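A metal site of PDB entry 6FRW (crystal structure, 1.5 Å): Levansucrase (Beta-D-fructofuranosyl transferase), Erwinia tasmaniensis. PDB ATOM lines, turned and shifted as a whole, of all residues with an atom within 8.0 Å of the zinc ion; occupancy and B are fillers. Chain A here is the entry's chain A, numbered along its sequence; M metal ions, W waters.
The side-chain carboxylate of Asp 48 is in hydrogen-bond range of the backbone NH of Gly 51 (3.3 Å).
The side-chain carboxylate (OD2) of Asp 50 binds the zinc ion (2.1 Å). OD2 of Asp 48 is bound to the zinc ion (2.2 Å). The zinc ion is bound by water W1, 2.3 Å away. The side-chain carboxylate (OD1) of Asp 52 is bound to the zinc ion.
Of the 13 residues printed, 3 come within 4 Å of the zinc ion. Along chain A the residues within 4 Å of the zinc ion span positions 48 to 52. The nearest printed residue that does not touch the zinc ion is Lys 406 (4.2 Å).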
ATOM      1  N   ARG A  47     -27.791  14.094 -21.626  1.00  0.00           N
ATOM      2  CA  ARG A  47     -27.919  12.660 -21.417  1.00  0.00           C
ATOM      3  C   ARG A  47     -29.386  12.264 -21.449  1.00  0.00           C
ATOM      4  O   ARG A  47     -30.292  13.110 -21.408  1.00  0.00           O
ATOM      5  CB  ARG A  47     -27.281  12.245 -20.080  1.00  0.00           C
ATOM      6  CG  ARG A  47     -27.663  13.133 -18.891  1.00  0.00           C
ATOM      7  CD  ARG A  47     -27.463  12.416 -17.548  1.00  0.00           C
ATOM      8  NE  ARG A  47     -28.530  11.452 -17.316  1.00  0.00           N
ATOM      9  CZ  ARG A  47     -29.083  11.172 -16.137  1.00  0.00           C
ATOM     10  NH1 ARG A  47     -30.056  10.265 -16.063  1.00  0.00           N
ATOM     11  NH2 ARG A  47     -28.677  11.791 -15.025  1.00  0.00           N
ATOM     12  N   ASP A  48     -29.633  10.951 -21.498  1.00  0.00           N
ATOM     13  CA  ASP A  48     -30.974  10.408 -21.387  1.00  0.00           C
ATOM     14  C   ASP A  48     -31.202   9.887 -19.965  1.00  0.00           C
ATOM     15  O   ASP A  48     -30.369  10.058 -19.082  1.00  0.00           O
ATOM     16  CB  ASP A  48     -31.225   9.319 -22.444  1.00  0.00           C
ATOM     17  CG  ASP A  48     -30.326   8.102 -22.278  1.00  0.00           C
ATOM     18  OD1 ASP A  48     -29.830   7.826 -21.169  1.00  0.00           O
ATOM     19  OD2 ASP A  48     -30.115   7.418 -23.296  1.00  0.00           O
ATOM     20  N   PHE A  49     -32.369   9.266 -19.747  1.00  0.00           N
ATOM     21  CA  PHE A  49     -32.773   8.964 -18.373  1.00  0.00           C
ATOM     22  C   PHE A  49     -31.985   7.825 -17.726  1.00  0.00           C
ATOM     23  O   PHE A  49     -32.192   7.577 -16.541  1.00  0.00           O
ATOM     24  CB  PHE A  49     -34.269   8.654 -18.324  1.00  0.00           C
ATOM     25  CG  PHE A  49     -35.130   9.877 -18.149  1.00  0.00           C
ATOM     26  CD1 PHE A  49     -35.070  10.623 -16.986  1.00  0.00           C
ATOM     27  CD2 PHE A  49     -36.003  10.272 -19.142  1.00  0.00           C
ATOM     28  CE1 PHE A  49     -35.861  11.751 -16.816  1.00  0.00           C
ATOM     29  CE2 PHE A  49     -36.810  11.390 -18.988  1.00  0.00           C
ATOM     30  CZ  PHE A  49     -36.741  12.126 -17.820  1.00  0.00           C
ATOM     31  N   ASP A  50     -31.077   7.153 -18.428  1.00  0.00           N
ATOM     32  CA  ASP A  50     -30.236   6.136 -17.793  1.00  0.00           C
ATOM     33  C   ASP A  50     -28.794   6.558 -17.587  1.00  0.00           C
ATOM     34  O   ASP A  50     -28.081   5.887 -16.813  1.00  0.00           O
ATOM     35  CB  ASP A  50     -30.242   4.839 -18.618  1.00  0.00           C
ATOM     36  CG  ASP A  50     -29.602   5.011 -19.981  1.00  0.00           C
ATOM     37  OD1 ASP A  50     -28.367   5.252 -20.035  1.00  0.00           O
ATOM     38  OD2 ASP A  50     -30.323   4.897 -20.992  1.00  0.00           O
ATOM     39  N   GLY A  51     -28.338   7.615 -18.241  1.00  0.00           N
ATOM     40  CA  GLY A  51     -26.976   8.070 -18.046  1.00  0.00           C
ATOM     41  C   GLY A  51     -26.211   8.248 -19.342  1.00  0.00           C
ATOM     42  O   GLY A  51     -25.210   8.972 -19.377  1.00  0.00           O
ATOM     43  N   ASP A  52     -26.670   7.583 -20.401  1.00  0.00           N
ATOM     44  CA  ASP A  52     -26.015   7.678 -21.697  1.00  0.00           C
ATOM     45  C   ASP A  52     -25.873   9.132 -22.139  1.00  0.00           C
ATOM     46  O   ASP A  52     -26.846   9.882 -22.143  1.00  0.00           O
ATOM     47  CB  ASP A  52     -26.815   6.928 -22.761  1.00  0.00           C
ATOM     48  CG  ASP A  52     -26.598   5.426 -22.705  1.00  0.00           C
ATOM     49  OD1 ASP A  52     -27.423   4.697 -23.293  1.00  0.00           O
ATOM     50  OD2 ASP A  52     -25.626   4.979 -22.069  1.00  0.00           O
ATOM     51  N   ILE A  53     -24.657   9.500 -22.518  1.00  0.00           N
ATOM     52  CA  ILE A  53     -24.436  10.804 -23.161  1.00  0.00           C
ATOM     53  C   ILE A  53     -24.938  10.733 -24.595  1.00  0.00           C
ATOM     54  O   ILE A  53     -24.598   9.825 -25.352  1.00  0.00           O
ATOM     55  CB  ILE A  53     -22.949  11.179 -23.105  1.00  0.00           C
ATOM     56  CG1 ILE A  53     -22.407  11.017 -21.672  1.00  0.00           C
ATOM     57  CG2 ILE A  53     -22.741  12.581 -23.628  1.00  0.00           C
ATOM     58  CD1 ILE A  53     -23.302  11.621 -20.594  1.00  0.00           C
ATOM     59  N   VAL A  54     -25.765  11.705 -24.990  1.00  0.00           N
ATOM     60  CA  VAL A  54     -26.419  11.657 -26.286  1.00  0.00           C
ATOM     61  C   VAL A  54     -26.068  12.911 -27.072  1.00  0.00           C
ATOM     62  O   VAL A  54     -26.076  14.020 -26.540  1.00  0.00           O
ATOM     63  CB  VAL A  54     -27.952  11.519 -26.144  1.00  0.00           C
ATOM     64  CG1 VAL A  54     -28.290  10.199 -25.472  1.00  0.00           C
ATOM     65  CG2 VAL A  54     -28.559  12.690 -25.372  1.00  0.00           C
ATOM     66  N   LYS A 206     -35.246   0.715 -14.527  1.00  0.00           N
ATOM     67  CA  LYS A 206     -36.066  -0.201 -15.309  1.00  0.00           C
ATOM     68  C   LYS A 206     -36.610  -1.343 -14.467  1.00  0.00           C
ATOM     69  O   LYS A 206     -37.551  -2.021 -14.894  1.00  0.00           O
ATOM     70  CB  LYS A 206     -35.258  -0.752 -16.494  1.00  0.00           C
ATOM     71  CG  LYS A 206     -34.990   0.260 -17.605  1.00  0.00           C
ATOM     72  CD  LYS A 206     -34.316  -0.411 -18.794  1.00  0.00           C
ATOM     73  CE  LYS A 206     -33.839   0.595 -19.830  1.00  0.00           C
ATOM     74  NZ  LYS A 206     -34.903   1.517 -20.302  1.00  0.00           N
ATOM     75  N   PRO A 354     -20.968   6.791 -18.226  1.00  0.00           N
ATOM     76  CA  PRO A 354     -21.029   5.327 -18.326  1.00  0.00           C
ATOM     77  C   PRO A 354     -20.028   4.718 -19.300  1.00  0.00           C
ATOM     78  O   PRO A 354     -19.826   3.502 -19.263  1.00  0.00           O
ATOM     79  CB  PRO A 354     -22.469   5.048 -18.783  1.00  0.00           C
ATOM     80  CG  PRO A 354     -23.226   6.282 -18.451  1.00  0.00           C
ATOM     81  CD  PRO A 354     -22.261   7.404 -18.617  1.00  0.00           C
ATOM     82  N   MET A 405     -22.231   8.885 -26.438  1.00  0.00           N
ATOM     83  CA  MET A 405     -22.280   7.433 -26.514  1.00  0.00           C
ATOM     84  C   MET A 405     -23.248   6.946 -27.584  1.00  0.00           C
ATOM     85  O   MET A 405     -23.046   5.860 -28.144  1.00  0.00           O
ATOM     86  CB  MET A 405     -22.681   6.861 -25.162  1.00  0.00           C
ATOM     87  CG  MET A 405     -21.612   7.126 -24.100  1.00  0.00           C
ATOM     88  SD  MET A 405     -22.197   6.850 -22.433  1.00  0.00           S
ATOM     89  CE  MET A 405     -22.684   5.128 -22.565  1.00  0.00           C
ATOM     90  N   LYS A 406     -24.279   7.723 -27.855  1.00  0.00           N
ATOM     91  CA  LYS A 406     -25.215   7.424 -28.927  1.00  0.00           C
ATOM     92  C   LYS A 406     -25.701   8.730 -29.536  1.00  0.00           C
ATOM     93  O   LYS A 406     -25.690   9.779 -28.894  1.00  0.00           O
ATOM     94  CB  LYS A 406     -26.408   6.598 -28.423  1.00  0.00           C
ATOM     95  CG  LYS A 406     -27.248   7.320 -27.387  1.00  0.00           C
ATOM     96  CD  LYS A 406     -28.304   6.412 -26.770  1.00  0.00           C
ATOM     97  CE  LYS A 406     -29.133   5.729 -27.827  1.00  0.00           C
ATOM     98  NZ  LYS A 406     -30.469   5.308 -27.302  1.00  0.00           N
ATOM     99  N   ILE A 408     -28.862  10.696 -31.503  1.00  0.00           N
ATOM    100  CA  ILE A 408     -30.310  10.710 -31.665  1.00  0.00           C
ATOM    101  C   ILE A 408     -30.618  11.552 -32.892  1.00  0.00           C
ATOM    102  O   ILE A 408     -30.276  12.743 -32.954  1.00  0.00           O
ATOM    103  CB  ILE A 408     -31.011  11.271 -30.421  1.00  0.00           C
ATOM    104  CG1 ILE A 408     -30.619  10.490 -29.167  1.00  0.00           C
ATOM    105  CG2 ILE A 408     -32.527  11.284 -30.603  1.00  0.00           C
ATOM    106  CD1 ILE A 408     -31.021   9.013 -29.187  1.00  0.00           C
HETATM  107 ZN    ZN M   1     -29.669   5.325 -22.904  1.00  0.00          ZN
HETATM  108  O   HOH W   1     -30.925   4.023 -24.355  1.00  0.00           O
